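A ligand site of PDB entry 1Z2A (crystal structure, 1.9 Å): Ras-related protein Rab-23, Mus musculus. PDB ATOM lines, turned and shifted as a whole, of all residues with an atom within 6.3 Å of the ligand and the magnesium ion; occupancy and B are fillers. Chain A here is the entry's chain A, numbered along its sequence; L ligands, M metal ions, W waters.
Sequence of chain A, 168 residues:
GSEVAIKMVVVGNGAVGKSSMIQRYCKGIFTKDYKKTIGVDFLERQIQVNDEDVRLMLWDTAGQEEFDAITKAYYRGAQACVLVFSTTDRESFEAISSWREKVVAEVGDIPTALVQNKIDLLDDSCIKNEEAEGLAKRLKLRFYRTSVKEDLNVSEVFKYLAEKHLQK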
ATOM      1  N   GLY A  12      13.599  18.179  16.109  1.00  0.00           N
ATOM      2  CA  GLY A  12      12.501  17.302  16.531  1.00  0.00           C
ATOM      3  C   GLY A  12      11.409  18.090  17.260  1.00  0.00           C
ATOM      4  O   GLY A  12      11.587  19.266  17.550  1.00  0.00           O
ATOM      5  N   ASN A  13      10.279  17.437  17.541  1.00  0.00           N
ATOM      6  CA  ASN A  13       9.180  18.069  18.310  1.00  0.00           C
ATOM      7  C   ASN A  13       9.613  18.606  19.680  1.00  0.00           C
ATOM      8  O   ASN A  13      10.637  18.192  20.230  1.00  0.00           O
ATOM      9  CB  ASN A  13       8.005  17.091  18.486  1.00  0.00           C
ATOM     10  CG  ASN A  13       7.079  17.049  17.284  1.00  0.00           C
ATOM     11  OD1 ASN A  13       7.418  17.531  16.190  1.00  0.00           O
ATOM     12  ND2 ASN A  13       5.901  16.445  17.462  1.00  0.00           N
ATOM     13  N   GLY A  14       8.831  19.531  20.225  1.00  0.00           N
ATOM     14  CA  GLY A  14       9.097  20.085  21.560  1.00  0.00           C
ATOM     15  C   GLY A  14       9.146  19.049  22.687  1.00  0.00           C
ATOM     16  O   GLY A  14       8.437  18.047  22.646  1.00  0.00           O
ATOM     17  N   ALA A  15      10.022  19.294  23.663  1.00  0.00           N
ATOM     18  CA  ALA A  15      10.117  18.509  24.907  1.00  0.00           C
ATOM     19  C   ALA A  15      10.729  17.092  24.760  1.00  0.00           C
ATOM     20  O   ALA A  15      10.762  16.322  25.731  1.00  0.00           O
ATOM     21  CB  ALA A  15       8.757  18.458  25.636  1.00  0.00           C
ATOM     22  N   VAL A  16      11.204  16.746  23.569  1.00  0.00           N
ATOM     23  CA  VAL A  16      11.876  15.447  23.355  1.00  0.00           C
ATOM     24  C   VAL A  16      13.239  15.330  24.061  1.00  0.00           C
ATOM     25  O   VAL A  16      13.731  14.225  24.258  1.00  0.00           O
ATOM     26  CB  VAL A  16      12.001  15.048  21.849  1.00  0.00           C
ATOM     27  CG1 VAL A  16      10.643  14.836  21.228  1.00  0.00           C
ATOM     28  CG2 VAL A  16      12.816  16.068  21.046  1.00  0.00           C
ATOM     29  N   GLY A  17      13.835  16.460  24.428  1.00  0.00           N
ATOM     30  CA  GLY A  17      15.122  16.490  25.131  1.00  0.00           C
ATOM     31  C   GLY A  17      16.295  17.025  24.326  1.00  0.00           C
ATOM     32  O   GLY A  17      17.439  16.697  24.619  1.00  0.00           O
ATOM     33  N   LYS A  18      16.008  17.856  23.321  1.00  0.00           N
ATOM     34  CA  LYS A  18      17.059  18.381  22.412  1.00  0.00           C
ATOM     35  C   LYS A  18      18.070  19.283  23.139  1.00  0.00           C
ATOM     36  O   LYS A  18      19.279  19.075  23.055  1.00  0.00           O
ATOM     37  CB  LYS A  18      16.443  19.126  21.215  1.00  0.00           C
ATOM     38  CG  LYS A  18      15.483  18.271  20.384  1.00  0.00           C
ATOM     39  CD  LYS A  18      15.012  18.989  19.117  1.00  0.00           C
ATOM     40  CE  LYS A  18      14.195  20.270  19.402  1.00  0.00           C
ATOM     41  NZ  LYS A  18      13.064  20.008  20.326  1.00  0.00           N
ATOM     42  N   SER A  19      17.563  20.292  23.850  1.00  0.00           N
ATOM     43  CA  SER A  19      18.430  21.207  24.608  1.00  0.00           C
ATOM     44  C   SER A  19      19.176  20.463  25.707  1.00  0.00           C
ATOM     45  O   SER A  19      20.366  20.731  25.954  1.00  0.00           O
ATOM     46  CB  SER A  19      17.609  22.356  25.211  1.00  0.00           C
ATOM     47  OG  SER A  19      16.886  23.063  24.201  1.00  0.00           O
ATOM     48  N   SER A  20      18.488  19.523  26.347  1.00  0.00           N
ATOM     49  CA  SER A  20      19.130  18.673  27.368  1.00  0.00           C
ATOM     50  C   SER A  20      20.317  17.911  26.763  1.00  0.00           C
ATOM     51  O   SER A  20      21.395  17.856  27.374  1.00  0.00           O
ATOM     52  CB  SER A  20      18.124  17.709  27.977  1.00  0.00           C
ATOM     53  OG  SER A  20      17.214  18.359  28.842  1.00  0.00           O
ATOM     54  N   MET A  21      20.124  17.349  25.580  1.00  0.00           N
ATOM     55  CA  MET A  21      21.174  16.590  24.891  1.00  0.00           C
ATOM     56  C   MET A  21      22.440  17.428  24.636  1.00  0.00           C
ATOM     57  O   MET A  21      23.566  16.961  24.872  1.00  0.00           O
ATOM     58  CB  MET A  21      20.645  15.984  23.590  1.00  0.00           C
ATOM     59  CG  MET A  21      21.608  15.038  22.889  1.00  0.00           C
ATOM     60  SD  MET A  21      20.912  14.328  21.390  1.00  0.00           S
ATOM     61  CE  MET A  21      22.016  12.956  21.106  1.00  0.00           C
ATOM     62  N   PHE A  30      22.927  17.595  33.716  1.00  0.00           N
ATOM     63  CA  PHE A  30      21.507  17.305  33.524  1.00  0.00           C
ATOM     64  C   PHE A  30      20.732  17.883  34.711  1.00  0.00           C
ATOM     65  O   PHE A  30      20.884  17.438  35.856  1.00  0.00           O
ATOM     66  CB  PHE A  30      21.245  15.790  33.403  1.00  0.00           C
ATOM     67  CG  PHE A  30      19.810  15.444  33.101  1.00  0.00           C
ATOM     68  CD1 PHE A  30      19.285  15.613  31.814  1.00  0.00           C
ATOM     69  CD2 PHE A  30      18.973  14.954  34.111  1.00  0.00           C
ATOM     70  CE1 PHE A  30      17.948  15.308  31.541  1.00  0.00           C
ATOM     71  CE2 PHE A  30      17.637  14.659  33.842  1.00  0.00           C
ATOM     72  CZ  PHE A  30      17.127  14.825  32.556  1.00  0.00           C
ATOM     73  N   THR A  31      19.899  18.887  34.440  1.00  0.00           N
ATOM     74  CA  THR A  31      19.093  19.516  35.495  1.00  0.00           C
ATOM     75  C   THR A  31      17.651  18.987  35.524  1.00  0.00           C
ATOM     76  O   THR A  31      17.246  18.269  34.604  1.00  0.00           O
ATOM     77  CB  THR A  31      19.103  21.052  35.395  1.00  0.00           C
ATOM     78  OG1 THR A  31      18.596  21.456  34.109  1.00  0.00           O
ATOM     79  CG2 THR A  31      20.524  21.589  35.550  1.00  0.00           C
ATOM     80  N   LYS A  32      16.896  19.348  36.557  1.00  0.00           N
ATOM     81  CA  LYS A  32      15.547  18.807  36.763  1.00  0.00           C
ATOM     82  C   LYS A  32      14.412  19.662  36.176  1.00  0.00           C
ATOM     83  O   LYS A  32      13.235  19.290  36.279  1.00  0.00           O
ATOM     84  CB  LYS A  32      15.294  18.516  38.254  1.00  0.00           C
ATOM     85  CG  LYS A  32      15.901  17.181  38.691  1.00  0.00           C
ATOM     86  CD  LYS A  32      15.671  16.841  40.161  1.00  0.00           C
ATOM     87  CE  LYS A  32      15.910  15.348  40.379  1.00  0.00           C
ATOM     88  NZ  LYS A  32      15.919  14.915  41.818  1.00  0.00           N
ATOM     89  N   ASP A  33      14.755  20.769  35.516  1.00  0.00           N
ATOM     90  CA  ASP A  33      13.767  21.697  34.949  1.00  0.00           C
ATOM     91  C   ASP A  33      12.809  21.038  33.961  1.00  0.00           C
ATOM     92  O   ASP A  33      13.181  20.090  33.275  1.00  0.00           O
ATOM     93  CB  ASP A  33      14.468  22.872  34.269  1.00  0.00           C
ATOM     94  CG  ASP A  33      15.429  23.606  35.200  1.00  0.00           C
ATOM     95  OD1 ASP A  33      15.270  24.823  35.384  1.00  0.00           O
ATOM     96  OD2 ASP A  33      16.343  22.960  35.743  1.00  0.00           O
ATOM     97  N   TYR A  34      11.563  21.523  33.914  1.00  0.00           N
ATOM     98  CA  TYR A  34      10.581  21.035  32.951  1.00  0.00           C
ATOM     99  C   TYR A  34      10.921  21.442  31.500  1.00  0.00           C
ATOM    100  O   TYR A  34      10.519  20.773  30.549  1.00  0.00           O
ATOM    101  CB  TYR A  34       9.158  21.480  33.327  1.00  0.00           C
ATOM    102  CG  TYR A  34       8.616  20.793  34.557  1.00  0.00           C
ATOM    103  CD1 TYR A  34       8.677  21.408  35.802  1.00  0.00           C
ATOM    104  CD2 TYR A  34       8.066  19.516  34.484  1.00  0.00           C
ATOM    105  CE1 TYR A  34       8.185  20.774  36.963  1.00  0.00           C
ATOM    106  CE2 TYR A  34       7.580  18.866  35.630  1.00  0.00           C
ATOM    107  CZ  TYR A  34       7.646  19.502  36.854  1.00  0.00           C
ATOM    108  OH  TYR A  34       7.157  18.872  37.985  1.00  0.00           O
ATOM    109  N   LYS A  35      11.652  22.536  31.359  1.00  0.00           N
ATOM    110  CA  LYS A  35      12.096  23.028  30.047  1.00  0.00           C
ATOM    111  C   LYS A  35      13.503  23.604  30.196  1.00  0.00           C
ATOM    112  O   LYS A  35      13.747  24.391  31.109  1.00  0.00           O
ATOM    113  CB  LYS A  35      11.135  24.085  29.510  1.00  0.00           C
ATOM    114  N   LYS A  36      14.417  23.225  29.291  1.00  0.00           N
ATOM    115  CA  LYS A  36      15.804  23.688  29.356  1.00  0.00           C
ATOM    116  C   LYS A  36      16.074  24.852  28.385  1.00  0.00           C
ATOM    117  O   LYS A  36      15.531  24.869  27.283  1.00  0.00           O
ATOM    118  CB  LYS A  36      16.781  22.541  29.060  1.00  0.00           C
ATOM    119  CG  LYS A  36      16.457  21.230  29.782  1.00  0.00           C
ATOM    120  CD  LYS A  36      16.888  21.267  31.220  1.00  0.00           C
ATOM    121  CE  LYS A  36      16.276  20.122  32.018  1.00  0.00           C
ATOM    122  NZ  LYS A  36      17.133  18.901  32.001  1.00  0.00           N
ATOM    123  N   THR A  37      16.907  25.789  28.805  1.00  0.00           N
ATOM    124  CA  THR A  37      17.245  26.955  27.966  1.00  0.00           C
ATOM    125  C   THR A  37      18.764  27.098  27.788  1.00  0.00           C
ATOM    126  O   THR A  37      19.529  26.868  28.723  1.00  0.00           O
ATOM    127  CB  THR A  37      16.662  28.275  28.556  1.00  0.00           C
ATOM    128  OG1 THR A  37      15.252  28.121  28.794  1.00  0.00           O
ATOM    129  CG2 THR A  37      16.852  29.431  27.575  1.00  0.00           C
ATOM    130  N   ASP A  60      21.108  25.186  18.988  1.00  0.00           N
ATOM    131  CA  ASP A  60      19.826  24.979  19.668  1.00  0.00           C
ATOM    132  C   ASP A  60      18.671  25.772  19.030  1.00  0.00           C
ATOM    133  O   ASP A  60      18.828  26.923  18.634  1.00  0.00           O
ATOM    134  CB  ASP A  60      19.942  25.349  21.150  1.00  0.00           C
ATOM    135  CG  ASP A  60      18.741  24.905  21.964  1.00  0.00           C
ATOM    136  OD1 ASP A  60      18.654  23.703  22.267  1.00  0.00           O
ATOM    137  OD2 ASP A  60      17.889  25.748  22.312  1.00  0.00           O
ATOM    138  N   THR A  61      17.501  25.145  18.966  1.00  0.00           N
ATOM    139  CA  THR A  61      16.309  25.718  18.325  1.00  0.00           C
ATOM    140  C   THR A  61      15.584  26.810  19.146  1.00  0.00           C
ATOM    141  O   THR A  61      14.682  27.493  18.615  1.00  0.00           O
ATOM    142  CB  THR A  61      15.281  24.613  18.013  1.00  0.00           C
ATOM    143  OG1 THR A  61      14.212  25.162  17.235  1.00  0.00           O
ATOM    144  CG2 THR A  61      14.718  24.032  19.285  1.00  0.00           C
ATOM    145  N   ALA A  62      15.953  26.955  20.413  1.00  0.00           N
ATOM    146  CA  ALA A  62      15.389  27.974  21.311  1.00  0.00           C
ATOM    147  C   ALA A  62      13.856  27.883  21.505  1.00  0.00           C
ATOM    148  O   ALA A  62      13.184  28.899  21.673  1.00  0.00           O
ATOM    149  CB  ALA A  62      15.809  29.391  20.866  1.00  0.00           C
ATOM    150  N   GLY A  63      13.333  26.660  21.471  1.00  0.00           N
ATOM    151  CA  GLY A  63      11.910  26.401  21.742  1.00  0.00           C
ATOM    152  C   GLY A  63      10.951  26.873  20.672  1.00  0.00           C
ATOM    153  O   GLY A  63       9.728  26.826  20.858  1.00  0.00           O
ATOM    154  N   GLU A  65      10.110  25.671  17.889  1.00  0.00           N
ATOM    155  CA  GLU A  65       9.311  24.617  17.248  1.00  0.00           C
ATOM    156  C   GLU A  65       7.872  24.556  17.775  1.00  0.00           C
ATOM    157  O   GLU A  65       6.982  24.029  17.103  1.00  0.00           O
ATOM    158  CB  GLU A  65       9.996  23.237  17.339  1.00  0.00           C
ATOM    159  CG  GLU A  65      10.092  22.626  18.751  1.00  0.00           C
ATOM    160  CD  GLU A  65      11.326  23.069  19.524  1.00  0.00           C
ATOM    161  OE1 GLU A  65      11.921  24.108  19.173  1.00  0.00           O
ATOM    162  OE2 GLU A  65      11.701  22.363  20.485  1.00  0.00           O
ATOM    163  N   ASN A 117      15.136   9.235  22.419  1.00  0.00           N
ATOM    164  CA  ASN A 117      15.499   9.681  23.764  1.00  0.00           C
ATOM    165  C   ASN A 117      14.494   9.198  24.821  1.00  0.00           C
ATOM    166  O   ASN A 117      13.400   8.719  24.477  1.00  0.00           O
ATOM    167  CB  ASN A 117      15.600  11.219  23.791  1.00  0.00           C
ATOM    168  CG  ASN A 117      16.361  11.752  25.004  1.00  0.00           C
ATOM    169  OD1 ASN A 117      16.082  12.861  25.490  1.00  0.00           O
ATOM    170  ND2 ASN A 117      17.309  10.980  25.499  1.00  0.00           N
ATOM    171  N   LYS A 118      14.870   9.347  26.100  1.00  0.00           N
ATOM    172  CA  LYS A 118      14.027   9.018  27.261  1.00  0.00           C
ATOM    173  C   LYS A 118      13.774   7.513  27.401  1.00  0.00           C
ATOM    174  O   LYS A 118      12.709   7.086  27.886  1.00  0.00           O
ATOM    175  CB  LYS A 118      12.705   9.813  27.269  1.00  0.00           C
ATOM    176  CG  LYS A 118      12.897  11.331  27.205  1.00  0.00           C
ATOM    177  CD  LYS A 118      11.653  12.069  27.652  1.00  0.00           C
ATOM    178  CE  LYS A 118      11.691  13.531  27.232  1.00  0.00           C
ATOM    179  NZ  LYS A 118      10.549  14.324  27.788  1.00  0.00           N
ATOM    180  N   ILE A 119      14.745   6.711  26.989  1.00  0.00           N
ATOM    181  CA  ILE A 119      14.622   5.255  27.047  1.00  0.00           C
ATOM    182  C   ILE A 119      14.602   4.735  28.486  1.00  0.00           C
ATOM    183  O   ILE A 119      14.289   3.569  28.730  1.00  0.00           O
ATOM    184  CB  ILE A 119      15.729   4.580  26.185  1.00  0.00           C
ATOM    185  CG1 ILE A 119      15.243   3.220  25.666  1.00  0.00           C
ATOM    186  CG2 ILE A 119      17.059   4.503  26.930  1.00  0.00           C
ATOM    187  CD1 ILE A 119      14.291   3.323  24.476  1.00  0.00           C
ATOM    188  N   ASP A 120      14.935   5.601  29.444  1.00  0.00           N
ATOM    189  CA  ASP A 120      14.810   5.270  30.873  1.00  0.00           C
ATOM    190  C   ASP A 120      13.343   5.130  31.316  1.00  0.00           C
ATOM    191  O   ASP A 120      13.053   4.586  32.387  1.00  0.00           O
ATOM    192  CB  ASP A 120      15.559   6.295  31.731  1.00  0.00           C
ATOM    193  CG  ASP A 120      15.105   7.733  31.474  1.00  0.00           C
ATOM    194  OD1 ASP A 120      15.360   8.266  30.368  1.00  0.00           O
ATOM    195  OD2 ASP A 120      14.506   8.330  32.387  1.00  0.00           O
ATOM    196  N   LEU A 121      12.429   5.635  30.478  1.00  0.00           N
ATOM    197  CA  LEU A 121      10.994   5.501  30.706  1.00  0.00           C
ATOM    198  C   LEU A 121      10.372   4.487  29.730  1.00  0.00           C
ATOM    199  O   LEU A 121       9.334   4.749  29.126  1.00  0.00           O
ATOM    200  CB  LEU A 121      10.288   6.868  30.580  1.00  0.00           C
ATOM    201  CG  LEU A 121      10.849   8.142  31.245  1.00  0.00           C
ATOM    202  CD1 LEU A 121      10.067   9.371  30.792  1.00  0.00           C
ATOM    203  CD2 LEU A 121      10.887   8.065  32.779  1.00  0.00           C
ATOM    204  N   THR A 146      18.611   6.151  23.396  1.00  0.00           N
ATOM    205  CA  THR A 146      19.352   7.138  24.178  1.00  0.00           C
ATOM    206  C   THR A 146      18.641   7.509  25.487  1.00  0.00           C
ATOM    207  O   THR A 146      17.406   7.551  25.547  1.00  0.00           O
ATOM    208  CB  THR A 146      19.604   8.409  23.289  1.00  0.00           C
ATOM    209  OG1 THR A 146      20.455   8.072  22.187  1.00  0.00           O
ATOM    210  CG2 THR A 146      20.199   9.554  24.062  1.00  0.00           C
ATOM    211  N   SER A 147      19.435   7.765  26.526  1.00  0.00           N
ATOM    212  CA  SER A 147      18.929   8.452  27.723  1.00  0.00           C
ATOM    213  C   SER A 147      19.842   9.620  28.073  1.00  0.00           C
ATOM    214  O   SER A 147      20.969   9.409  28.557  1.00  0.00           O
ATOM    215  CB  SER A 147      18.818   7.483  28.914  1.00  0.00           C
ATOM    216  OG  SER A 147      18.224   8.126  30.043  1.00  0.00           O
ATOM    217  N   VAL A 148      19.389  10.844  27.813  1.00  0.00           N
ATOM    218  CA  VAL A 148      20.147  12.042  28.184  1.00  0.00           C
ATOM    219  C   VAL A 148      20.298  12.084  29.724  1.00  0.00           C
ATOM    220  O   VAL A 148      21.379  12.398  30.256  1.00  0.00           O
ATOM    221  CB  VAL A 148      19.525  13.368  27.637  1.00  0.00           C
ATOM    222  CG1 VAL A 148      20.252  14.593  28.184  1.00  0.00           C
ATOM    223  CG2 VAL A 148      19.571  13.395  26.116  1.00  0.00           C
ATOM    224  N   LYS A 149      19.207  11.727  30.407  1.00  0.00           N
ATOM    225  CA  LYS A 149      19.168  11.671  31.875  1.00  0.00           C
ATOM    226  C   LYS A 149      20.286  10.803  32.468  1.00  0.00           C
ATOM    227  O   LYS A 149      21.021  11.242  33.367  1.00  0.00           O
ATOM    228  CB  LYS A 149      17.784  11.189  32.368  1.00  0.00           C
ATOM    229  CG  LYS A 149      17.643  11.113  33.897  1.00  0.00           C
ATOM    230  CD  LYS A 149      16.280  10.596  34.321  1.00  0.00           C
ATOM    231  CE  LYS A 149      16.237  10.316  35.828  1.00  0.00           C
ATOM    232  NZ  LYS A 149      14.904   9.801  36.241  1.00  0.00           N
ATOM    233  N   GLU A 150      20.449   9.586  31.957  1.00  0.00           N
ATOM    234  CA  GLU A 150      21.480   8.669  32.448  1.00  0.00           C
ATOM    235  C   GLU A 150      22.817   8.727  31.671  1.00  0.00           C
ATOM    236  O   GLU A 150      23.720   7.922  31.934  1.00  0.00           O
ATOM    237  CB  GLU A 150      20.941   7.231  32.528  1.00  0.00           C
ATOM    238  CG  GLU A 150      19.706   7.066  33.444  1.00  0.00           C
ATOM    239  CD  GLU A 150      19.977   7.452  34.904  1.00  0.00           C
ATOM    240  OE1 GLU A 150      21.125   7.269  35.374  1.00  0.00           O
ATOM    241  OE2 GLU A 150      19.031   7.928  35.588  1.00  0.00           O
HETATM  242  P1  LIG L   1      13.451  20.158  24.019  1.00  0.00           P
HETATM  243  O1  LIG L   1      12.187  20.998  24.036  1.00  0.00           O
HETATM  244  O2  LIG L   1      13.356  19.177  22.898  1.00  0.00           O
HETATM  245  O3  LIG L   1      14.672  21.044  23.878  1.00  0.00           O
HETATM  246  O4  LIG L   1      13.527  19.319  25.394  1.00  0.00           O
HETATM  247  P2  LIG L   1      14.194  19.800  26.773  1.00  0.00           P
HETATM  248  O5  LIG L   1      13.767  21.189  27.168  1.00  0.00           O
HETATM  249  O6  LIG L   1      15.710  19.704  26.683  1.00  0.00           O
HETATM  250  O7  LIG L   1      13.650  18.707  27.824  1.00  0.00           O
HETATM  251  C1  LIG L   1      12.251  18.594  28.092  1.00  0.00           C
HETATM  252  C2  LIG L   1      12.034  17.818  29.394  1.00  0.00           C
HETATM  253  O8  LIG L   1      12.399  16.455  29.202  1.00  0.00           O
HETATM  254  C3  LIG L   1      12.880  18.346  30.531  1.00  0.00           C
HETATM  255  O9  LIG L   1      12.112  18.235  31.733  1.00  0.00           O
HETATM  256  C4  LIG L   1      14.062  17.385  30.569  1.00  0.00           C
HETATM  257  O10 LIG L   1      14.685  17.281  31.840  1.00  0.00           O
HETATM  258  C5  LIG L   1      13.399  16.085  30.154  1.00  0.00           C
HETATM  259  N1  LIG L   1      14.358  15.092  29.588  1.00  0.00           N
HETATM  260  C6  LIG L   1      15.301  15.305  28.649  1.00  0.00           C
HETATM  261  N2  LIG L   1      15.982  14.160  28.378  1.00  0.00           N
HETATM  262  C7  LIG L   1      15.470  13.179  29.162  1.00  0.00           C
HETATM  263  C8  LIG L   1      15.715  11.728  29.386  1.00  0.00           C
HETATM  264  O11 LIG L   1      16.608  11.090  28.764  1.00  0.00           O
HETATM  265  N3  LIG L   1      14.949  11.095  30.304  1.00  0.00           N
HETATM  266  C9  LIG L   1      13.978  11.731  30.992  1.00  0.00           C
HETATM  267  N4  LIG L   1      13.252  11.026  31.888  1.00  0.00           N
HETATM  268  N5  LIG L   1      13.705  13.047  30.840  1.00  0.00           N
HETATM  269  C10 LIG L   1      14.397  13.809  29.951  1.00  0.00           C
HETATM  270 MG    MG M   1      14.840  23.108  23.620  1.00  0.00          MG
HETATM  271  O   HOH W   1      15.225  25.349  23.342  1.00  0.00           O
HETATM  272  O   HOH W   2      15.588  22.718  21.708  1.00  0.00           O
HETATM  273  O   HOH W   3      13.554  16.224  34.204  1.00  0.00           O
HETATM  274  O   HOH W   4      12.786  23.213  22.820  1.00  0.00           O
HETATM  275  O   HOH W   5      10.454  22.201  25.732  1.00  0.00           O
HETATM  276  O   HOH W   6       9.847  16.263  32.161  1.00  0.00           O
HETATM  277  O   HOH W   7      14.216  23.409  25.588  1.00  0.00           O
HETATM  278  O   HOH W   8      10.536  13.798  30.479  1.00  0.00           O
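N of Lys 36 sits at hydrogen-bond distance from O5 of the ligand (3.0 Å).
An oxygen (O11) of the ligand lies within hydrogen-bond range of the backbone NH (N) of Val 148, 2.9 Å away.
N of Lys 149 lies within hydrogen-bond range of O11 of the ligand (3.1 Å).
The backbone NH (N) of Ser 19 is in hydrogen-bond range of an oxygen (O6) of the ligand (3.4 Å).
The backbone NH of Lys 18 lies within hydrogen-bond range of an oxygen (O2) of the ligand (3.0 Å).
The side-chain carboxylate (OD1) of Asp 120 lies within hydrogen-bond range of a nitrogen (N3) of the ligand, 2.9 Å away.
An oxygen (O4) of the ligand lies within hydrogen-bond range of the backbone NH (N) of Gly 17 (3.0 Å).
OD1 of Asn 117 lies close to N2 of the ligand.
O10 of the ligand lies within hydrogen-bond range of NZ of Lys 36, 2.9 Å away.
The backbone carbonyl oxygen (O) of Tyr 34 lies within hydrogen-bond range of an oxygen (O9) of the ligand (3.2 Å).
An oxygen (O2) of the ligand lies within salt-bridge range of the side-chain amino group of Lys 18.
An oxygen (O2) of the ligand sits at hydrogen-bond distance from the backbone NH of Val 16, 3.3 Å away.
An oxygen (O6) of the ligand sits at hydrogen-bond distance from the side-chain hydroxyl (OG) of Ser 20 (3.0 Å).
O9 of the ligand sits at hydrogen-bond distance from O of Asp 33 (2.6 Å).
The backbone NH (N) of Ser 20 sits at hydrogen-bond distance from an oxygen (O6) of the ligand (2.8 Å).
NZ of Lys 118 sits at hydrogen-bond distance from O8 of the ligand, 3.2 Å away.
N of Ala 15 is in hydrogen-bond range of O1 of the ligand, 2.8 Å away.
The backbone carbonyl oxygen (O) of Asn 13 is in hydrogen-bond range of the side-chain amino group (NZ) of Lys 18 (3.0 Å).
O of Ala 15 lies within hydrogen-bond range of NZ of Lys 118, at 2.9 Å.
The side-chain amide oxygen (OD1) of Asn 117 lies close to the backbone carbonyl oxygen (O) of Val 16 (3.0 Å).
The side-chain hydroxyl (OG) of Ser 147 is in hydrogen-bond range of the side-chain carboxylate (OD1) of Asp 120 (2.9 Å).
NZ of Lys 36 lies close to OG of Ser 20 (3.2 Å).
The backbone NH of Val 148 sits close to the side-chain amide nitrogen of Asn 117 (3.1 Å).
The side-chain carboxylate (OE1) of Glu 65 sits close to the side-chain hydroxyl (OG1) of Thr 61.
OG of Ser 19 lies close to OD1 of Asp 60 (2.7 Å).
Merely in contact with the ligand: Phe 30, Ser 147, Leu 121, Lys 35, Glu 65, Gly 14, Thr 31 and Asn 13.
Hydrophobic or aromatic side chains within 4 Å of the ligand: Val 16, Phe 30, Leu 121 and Val 148.
The nearest printed residue that does not touch the ligand is Lys 32 (4.8 Å).
One residue has an atom within 4 Å of the magnesium ion: Ser 19.
The magnesium ion is bound by water W7 (2.1 Å), an oxygen (O3) of the ligand (2.1 Å), water W2 (2.1 Å), the side-chain hydroxyl of Ser 19 (2.1 Å), water W4 (2.2 Å) and water W1 (2.3 Å).
Water W7 bridges the backbone carbonyl oxygen of Lys 36 and an oxygen (O5) of the ligand.
Water W4 bridges O1 of the ligand (2.6 Å) and OE2 of Glu 65 (2.7 Å).
Water W1 lies within hydrogen-bond range of OD2 of Asp 60 (2.9 Å), N of Gly 63 (3.0 Å) and N of Ala 62 (3.4 Å).
Water W8 lies within hydrogen-bond range of NZ of Lys 118 and N5 of the ligand.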
